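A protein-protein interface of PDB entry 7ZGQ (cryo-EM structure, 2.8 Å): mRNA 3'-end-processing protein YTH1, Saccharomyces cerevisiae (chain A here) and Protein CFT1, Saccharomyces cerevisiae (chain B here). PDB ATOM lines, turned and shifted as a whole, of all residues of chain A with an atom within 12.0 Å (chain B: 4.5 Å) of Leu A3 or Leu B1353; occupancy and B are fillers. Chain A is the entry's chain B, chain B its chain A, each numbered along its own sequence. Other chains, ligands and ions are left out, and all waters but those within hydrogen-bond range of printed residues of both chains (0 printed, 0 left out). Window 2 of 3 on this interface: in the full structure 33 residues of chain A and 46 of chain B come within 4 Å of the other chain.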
ATOM      1  N   MET A   1      -7.896  20.421 -11.798  1.00  0.00           N
ATOM      2  CA  MET A   1      -8.280  21.412 -12.796  1.00  0.00           C
ATOM      3  C   MET A   1      -9.708  21.886 -12.568  1.00  0.00           C
ATOM      4  O   MET A   1     -10.629  21.479 -13.277  1.00  0.00           O
ATOM      5  CB  MET A   1      -8.136  20.839 -14.207  1.00  0.00           C
ATOM      6  N   SER A   2      -9.890  22.746 -11.571  1.00  0.00           N
ATOM      7  CA  SER A   2     -11.193  23.302 -11.238  1.00  0.00           C
ATOM      8  C   SER A   2     -11.210  24.783 -11.583  1.00  0.00           C
ATOM      9  O   SER A   2     -10.347  25.540 -11.130  1.00  0.00           O
ATOM     10  CB  SER A   2     -11.515  23.100  -9.756  1.00  0.00           C
ATOM     11  OG  SER A   2     -12.686  23.807  -9.387  1.00  0.00           O
ATOM     12  N   LEU A   3     -12.190  25.187 -12.394  1.00  0.00           N
ATOM     13  CA  LEU A   3     -12.347  26.602 -12.708  1.00  0.00           C
ATOM     14  C   LEU A   3     -12.792  27.388 -11.484  1.00  0.00           C
ATOM     15  O   LEU A   3     -12.380  28.536 -11.287  1.00  0.00           O
ATOM     16  CB  LEU A   3     -13.355  26.777 -13.845  1.00  0.00           C
ATOM     17  CG  LEU A   3     -13.112  26.002 -15.141  1.00  0.00           C
ATOM     18  CD1 LEU A   3     -14.257  26.224 -16.117  1.00  0.00           C
ATOM     19  CD2 LEU A   3     -11.788  26.400 -15.768  1.00  0.00           C
ATOM     20  N   ILE A   4     -13.634  26.779 -10.649  1.00  0.00           N
ATOM     21  CA  ILE A   4     -14.298  27.514  -9.580  1.00  0.00           C
ATOM     22  C   ILE A   4     -13.323  27.820  -8.449  1.00  0.00           C
ATOM     23  O   ILE A   4     -13.339  28.915  -7.876  1.00  0.00           O
ATOM     24  CB  ILE A   4     -15.514  26.715  -9.090  1.00  0.00           C
ATOM     25  CG1 ILE A   4     -16.318  26.249 -10.306  1.00  0.00           C
ATOM     26  CG2 ILE A   4     -16.356  27.553  -8.137  1.00  0.00           C
ATOM     27  CD1 ILE A   4     -17.392  27.178 -10.738  1.00  0.00           C
ATOM     28  N   HIS A   5     -12.467  26.860  -8.109  1.00  0.00           N
ATOM     29  CA  HIS A   5     -11.426  27.034  -7.098  1.00  0.00           C
ATOM     30  C   HIS A   5     -10.101  26.652  -7.738  1.00  0.00           C
ATOM     31  O   HIS A   5      -9.583  25.549  -7.512  1.00  0.00           O
ATOM     32  CB  HIS A   5     -11.702  26.192  -5.852  1.00  0.00           C
ATOM     33  CG  HIS A   5     -13.084  26.356  -5.303  1.00  0.00           C
ATOM     34  ND1 HIS A   5     -13.515  27.524  -4.712  1.00  0.00           N
ATOM     35  CD2 HIS A   5     -14.131  25.499  -5.250  1.00  0.00           C
ATOM     36  CE1 HIS A   5     -14.768  27.380  -4.322  1.00  0.00           C
ATOM     37  NE2 HIS A   5     -15.166  26.161  -4.637  1.00  0.00           N
ATOM     38  N   PRO A   6      -9.528  27.535  -8.554  1.00  0.00           N
ATOM     39  CA  PRO A   6      -8.292  27.189  -9.265  1.00  0.00           C
ATOM     40  C   PRO A   6      -7.159  26.874  -8.301  1.00  0.00           C
ATOM     41  O   PRO A   6      -7.024  27.494  -7.244  1.00  0.00           O
ATOM     42  CB  PRO A   6      -7.996  28.444 -10.094  1.00  0.00           C
ATOM     43  CG  PRO A   6      -8.748  29.541  -9.416  1.00  0.00           C
ATOM     44  CD  PRO A   6      -9.980  28.902  -8.860  1.00  0.00           C
ATOM     45  N   ASP A   7      -6.342  25.895  -8.679  1.00  0.00           N
ATOM     46  CA  ASP A   7      -5.212  25.477  -7.858  1.00  0.00           C
ATOM     47  C   ASP A   7      -4.184  26.600  -7.810  1.00  0.00           C
ATOM     48  O   ASP A   7      -3.505  26.876  -8.804  1.00  0.00           O
ATOM     49  CB  ASP A   7      -4.600  24.195  -8.415  1.00  0.00           C
ATOM     50  CG  ASP A   7      -3.728  23.477  -7.403  1.00  0.00           C
ATOM     51  OD1 ASP A   7      -3.510  24.029  -6.304  1.00  0.00           O
ATOM     52  OD2 ASP A   7      -3.259  22.360  -7.708  1.00  0.00           O
ATOM     53  N   THR A   8      -4.072  27.250  -6.653  1.00  0.00           N
ATOM     54  CA  THR A   8      -3.160  28.367  -6.473  1.00  0.00           C
ATOM     55  C   THR A   8      -2.151  28.153  -5.357  1.00  0.00           C
ATOM     56  O   THR A   8      -1.251  28.986  -5.197  1.00  0.00           O
ATOM     57  CB  THR A   8      -3.947  29.656  -6.185  1.00  0.00           C
ATOM     58  OG1 THR A   8      -4.873  29.420  -5.118  1.00  0.00           O
ATOM     59  CG2 THR A   8      -4.721  30.088  -7.417  1.00  0.00           C
ATOM     60  N   VAL B 516     -18.326  32.097 -11.824  1.00  0.00           N
ATOM     61  CA  VAL B 516     -18.453  31.037 -12.814  1.00  0.00           C
ATOM     62  C   VAL B 516     -19.244  29.902 -12.186  1.00  0.00           C
ATOM     63  O   VAL B 516     -19.140  29.656 -10.978  1.00  0.00           O
ATOM     64  CB  VAL B 516     -17.065  30.572 -13.295  1.00  0.00           C
ATOM     65  CG1 VAL B 516     -17.147  29.245 -14.025  1.00  0.00           C
ATOM     66  CG2 VAL B 516     -16.449  31.626 -14.188  1.00  0.00           C
ATOM     67  N   ASN B 535     -19.735  19.786 -20.054  1.00  0.00           N
ATOM     68  CA  ASN B 535     -18.465  20.274 -19.513  1.00  0.00           C
ATOM     69  C   ASN B 535     -18.264  21.760 -19.790  1.00  0.00           C
ATOM     70  O   ASN B 535     -17.132  22.231 -19.913  1.00  0.00           O
ATOM     71  CB  ASN B 535     -17.278  19.470 -20.053  1.00  0.00           C
ATOM     72  CG  ASN B 535     -17.491  17.975 -19.954  1.00  0.00           C
ATOM     73  OD1 ASN B 535     -17.579  17.280 -20.966  1.00  0.00           O
ATOM     74  ND2 ASN B 535     -17.570  17.468 -18.730  1.00  0.00           N
ATOM     75  N   GLU B 536     -19.355  22.512 -19.882  1.00  0.00           N
ATOM     76  CA  GLU B 536     -19.307  23.928 -20.211  1.00  0.00           C
ATOM     77  C   GLU B 536     -19.760  24.753 -19.016  1.00  0.00           C
ATOM     78  O   GLU B 536     -20.855  24.538 -18.486  1.00  0.00           O
ATOM     79  CB  GLU B 536     -20.182  24.237 -21.426  1.00  0.00           C
ATOM     80  CG  GLU B 536     -20.282  25.716 -21.752  1.00  0.00           C
ATOM     81  CD  GLU B 536     -21.655  26.109 -22.254  1.00  0.00           C
ATOM     82  OE1 GLU B 536     -22.649  25.815 -21.558  1.00  0.00           O
ATOM     83  OE2 GLU B 536     -21.741  26.713 -23.344  1.00  0.00           O
ATOM     84  N   TYR B 537     -18.920  25.692 -18.599  1.00  0.00           N
ATOM     85  CA  TYR B 537     -19.252  26.645 -17.553  1.00  0.00           C
ATOM     86  C   TYR B 537     -19.581  27.995 -18.178  1.00  0.00           C
ATOM     87  O   TYR B 537     -19.203  28.287 -19.314  1.00  0.00           O
ATOM     88  CB  TYR B 537     -18.099  26.791 -16.556  1.00  0.00           C
ATOM     89  CG  TYR B 537     -17.921  25.616 -15.619  1.00  0.00           C
ATOM     90  CD1 TYR B 537     -17.635  24.348 -16.106  1.00  0.00           C
ATOM     91  CD2 TYR B 537     -18.031  25.778 -14.246  1.00  0.00           C
ATOM     92  CE1 TYR B 537     -17.469  23.276 -15.254  1.00  0.00           C
ATOM     93  CE2 TYR B 537     -17.867  24.710 -13.386  1.00  0.00           C
ATOM     94  CZ  TYR B 537     -17.585  23.462 -13.895  1.00  0.00           C
ATOM     95  OH  TYR B 537     -17.420  22.394 -13.042  1.00  0.00           O
ATOM     96  N   SER B 538     -20.298  28.819 -17.422  1.00  0.00           N
ATOM     97  CA  SER B 538     -20.734  30.118 -17.907  1.00  0.00           C
ATOM     98  C   SER B 538     -20.510  31.181 -16.843  1.00  0.00           C
ATOM     99  O   SER B 538     -20.490  30.891 -15.645  1.00  0.00           O
ATOM    100  CB  SER B 538     -22.211  30.093 -18.313  1.00  0.00           C
ATOM    101  OG  SER B 538     -22.985  29.406 -17.350  1.00  0.00           O
ATOM    102  N   LEU B 539     -20.340  32.419 -17.299  1.00  0.00           N
ATOM    103  CA  LEU B 539     -20.218  33.559 -16.402  1.00  0.00           C
ATOM    104  C   LEU B 539     -21.608  34.032 -15.999  1.00  0.00           C
ATOM    105  O   LEU B 539     -22.430  34.365 -16.859  1.00  0.00           O
ATOM    106  CB  LEU B 539     -19.445  34.690 -17.074  1.00  0.00           C
ATOM    107  CG  LEU B 539     -17.927  34.678 -16.912  1.00  0.00           C
ATOM    108  CD1 LEU B 539     -17.302  35.755 -17.775  1.00  0.00           C
ATOM    109  CD2 LEU B 539     -17.557  34.877 -15.457  1.00  0.00           C
ATOM    110  N   LEU B1230      -9.766  33.961 -13.351  1.00  0.00           N
ATOM    111  CA  LEU B1230     -10.238  32.899 -14.221  1.00  0.00           C
ATOM    112  C   LEU B1230      -9.071  32.286 -14.980  1.00  0.00           C
ATOM    113  O   LEU B1230      -8.183  33.011 -15.444  1.00  0.00           O
ATOM    114  CB  LEU B1230     -11.280  33.432 -15.215  1.00  0.00           C
ATOM    115  CG  LEU B1230     -12.406  32.474 -15.597  1.00  0.00           C
ATOM    116  CD1 LEU B1230     -12.943  31.788 -14.358  1.00  0.00           C
ATOM    117  CD2 LEU B1230     -13.514  33.215 -16.324  1.00  0.00           C
ATOM    118  N   PRO B1231      -9.039  30.961 -15.117  1.00  0.00           N
ATOM    119  CA  PRO B1231      -7.993  30.333 -15.930  1.00  0.00           C
ATOM    120  C   PRO B1231      -8.098  30.753 -17.387  1.00  0.00           C
ATOM    121  O   PRO B1231      -9.187  30.992 -17.913  1.00  0.00           O
ATOM    122  CB  PRO B1231      -8.260  28.833 -15.761  1.00  0.00           C
ATOM    123  CG  PRO B1231      -9.067  28.721 -14.517  1.00  0.00           C
ATOM    124  CD  PRO B1231      -9.890  29.965 -14.446  1.00  0.00           C
ATOM    125  N   MET B1350     -11.284  33.233 -22.971  1.00  0.00           N
ATOM    126  CA  MET B1350     -12.334  32.858 -22.038  1.00  0.00           C
ATOM    127  C   MET B1350     -12.997  31.532 -22.388  1.00  0.00           C
ATOM    128  O   MET B1350     -13.961  31.142 -21.722  1.00  0.00           O
ATOM    129  CB  MET B1350     -13.393  33.959 -21.965  1.00  0.00           C
ATOM    130  CG  MET B1350     -12.970  35.177 -21.163  1.00  0.00           C
ATOM    131  SD  MET B1350     -14.265  35.732 -20.040  1.00  0.00           S
ATOM    132  CE  MET B1350     -15.725  35.321 -20.990  1.00  0.00           C
ATOM    133  N   ARG B1351     -12.509  30.833 -23.410  1.00  0.00           N
ATOM    134  CA  ARG B1351     -13.061  29.533 -23.769  1.00  0.00           C
ATOM    135  C   ARG B1351     -12.630  28.425 -22.818  1.00  0.00           C
ATOM    136  O   ARG B1351     -12.987  27.264 -23.046  1.00  0.00           O
ATOM    137  CB  ARG B1351     -12.672  29.168 -25.202  1.00  0.00           C
ATOM    138  CG  ARG B1351     -13.303  30.070 -26.245  1.00  0.00           C
ATOM    139  CD  ARG B1351     -13.452  29.368 -27.578  1.00  0.00           C
ATOM    140  NE  ARG B1351     -14.222  30.170 -28.520  1.00  0.00           N
ATOM    141  CZ  ARG B1351     -14.408  29.856 -29.795  1.00  0.00           C
ATOM    142  NH1 ARG B1351     -13.886  28.760 -30.320  1.00  0.00           N
ATOM    143  NH2 ARG B1351     -15.134  30.663 -30.562  1.00  0.00           N
ATOM    144  N   SER B1352     -11.872  28.749 -21.769  1.00  0.00           N
ATOM    145  CA  SER B1352     -11.577  27.768 -20.735  1.00  0.00           C
ATOM    146  C   SER B1352     -12.831  27.343 -19.986  1.00  0.00           C
ATOM    147  O   SER B1352     -12.831  26.289 -19.343  1.00  0.00           O
ATOM    148  CB  SER B1352     -10.545  28.327 -19.756  1.00  0.00           C
ATOM    149  OG  SER B1352     -11.098  29.368 -18.972  1.00  0.00           O
ATOM    150  N   LEU B1353     -13.898  28.141 -20.053  1.00  0.00           N
ATOM    151  CA  LEU B1353     -15.174  27.761 -19.465  1.00  0.00           C
ATOM    152  C   LEU B1353     -15.878  26.664 -20.251  1.00  0.00           C
ATOM    153  O   LEU B1353     -16.840  26.082 -19.741  1.00  0.00           O
ATOM    154  CB  LEU B1353     -16.089  28.982 -19.362  1.00  0.00           C
ATOM    155  CG  LEU B1353     -15.516  30.211 -18.658  1.00  0.00           C
ATOM    156  CD1 LEU B1353     -16.488  31.373 -18.742  1.00  0.00           C
ATOM    157  CD2 LEU B1353     -15.186  29.888 -17.213  1.00  0.00           C
ATOM    158  N   CYS B1354     -15.428  26.373 -21.471  1.00  0.00           N
ATOM    159  CA  CYS B1354     -16.036  25.329 -22.282  1.00  0.00           C
ATOM    160  C   CYS B1354     -15.504  23.941 -21.958  1.00  0.00           C
ATOM    161  O   CYS B1354     -16.068  22.952 -22.438  1.00  0.00           O
ATOM    162  CB  CYS B1354     -15.818  25.626 -23.768  1.00  0.00           C
ATOM    163  SG  CYS B1354     -16.690  27.088 -24.373  1.00  0.00           S
ATOM    164  N   GLN B1355     -14.438  23.841 -21.164  1.00  0.00           N
ATOM    165  CA  GLN B1355     -13.840  22.562 -20.780  1.00  0.00           C
ATOM    166  C   GLN B1355     -13.667  22.568 -19.264  1.00  0.00           C
ATOM    167  O   GLN B1355     -12.609  22.940 -18.750  1.00  0.00           O
ATOM    168  CB  GLN B1355     -12.515  22.341 -21.500  1.00  0.00           C
ATOM    169  CG  GLN B1355     -11.780  23.625 -21.845  1.00  0.00           C
ATOM    170  CD  GLN B1355     -10.373  23.374 -22.344  1.00  0.00           C
ATOM    171  OE1 GLN B1355      -9.926  22.230 -22.430  1.00  0.00           O
ATOM    172  NE2 GLN B1355      -9.663  24.447 -22.675  1.00  0.00           N
ATOM    173  N   GLY B1356     -14.708  22.151 -18.550  1.00  0.00           N
ATOM    174  CA  GLY B1356     -14.693  22.134 -17.101  1.00  0.00           C
ATOM    175  C   GLY B1356     -14.841  20.724 -16.561  1.00  0.00           C
ATOM    176  O   GLY B1356     -15.510  19.880 -17.161  1.00  0.00           O
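The side-chain hydroxyl (OG) of Ser A2 sits close to the backbone NH (N) of Ile A4.
N of Tyr B537 lies within hydrogen-bond range of O of Leu B1353 (2.4 Å).
The side-chain hydroxyl of Ser B1352 sits at hydrogen-bond distance from the backbone carbonyl oxygen of Pro B1231, 2.7 Å away.
CG of Tyr B537 touches CD1 of Leu A3, 3.7 Å away.
CD2 of Leu A3 touches CG of Pro B1231, at 3.8 Å.
CD1 of Leu A3 touches O of Ser B1352 (3.5 Å).
Leu A3 touches Leu B1353.
O of Val B516 touches CD1 of Ile A4, at 3.0 Å.
Tyr B537 touches Ile A4 (CE2 to CD1, 3.7 Å).
Met A1 touches none of the printed residues of chain B.
Leu A3 touches just these residues of chain B: Tyr B537 (3.7 Å), Pro B1231 (3.8 Å), Ser B1352 (3.5 Å) and Leu B1353 (3.8 Å).
Of the printed residues of chain B, Ile A4 touches Val B516 and Tyr B537.
No residue of chain A comes within 4 Å of Glu B536.
Tyr B537 touches just these residues of chain A: Leu A3 (3.7 Å) and Ile A4 (3.7 Å).
No residue of chain A comes within 4 Å of Ser B538.
No residue of chain A comes within 4 Å of Leu B539.
No residue of chain A comes within 4 Å of Leu B1230.
Of chain A, only Leu A3 comes within 4 Å of Pro B1231.
Ser B1352 touches one residue of chain A.
Of chain A, only Leu A3 (3.8 Å) comes within 4 Å of Leu B1353.
No residue of chain A comes within 4 Å of Cys B1354.
No residue of chain A comes within 4 Å of Gly B1356.
The nearest residue of chain A that does not touch Leu B1353 is Ile A4 (7.4 Å).
Printed residues of chain A that touch a printed residue of chain B: Leu A3 and Ile A4.
Along chain A the printed residues that touch a printed residue of chain B span positions 3 to 4.
Of the 15 printed residues of chain B, 5 touch a printed residue of chain A.
Printed residues of chain B that touch a printed residue of chain A: Val B516, Tyr B537, Pro B1231, Ser B1352 and Leu B1353.
Hydrophobic or aromatic side chains of chain B that line the printed part of chain A: Val B516, Tyr B537, Pro B1231 and Leu B1353.
Among the printed residues, 6 pairs touch across the chains.
Among the printed residues, no Asp or Glu carboxylate lies within 4 Å of a Lys or Arg side-chain nitrogen of the other chain.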
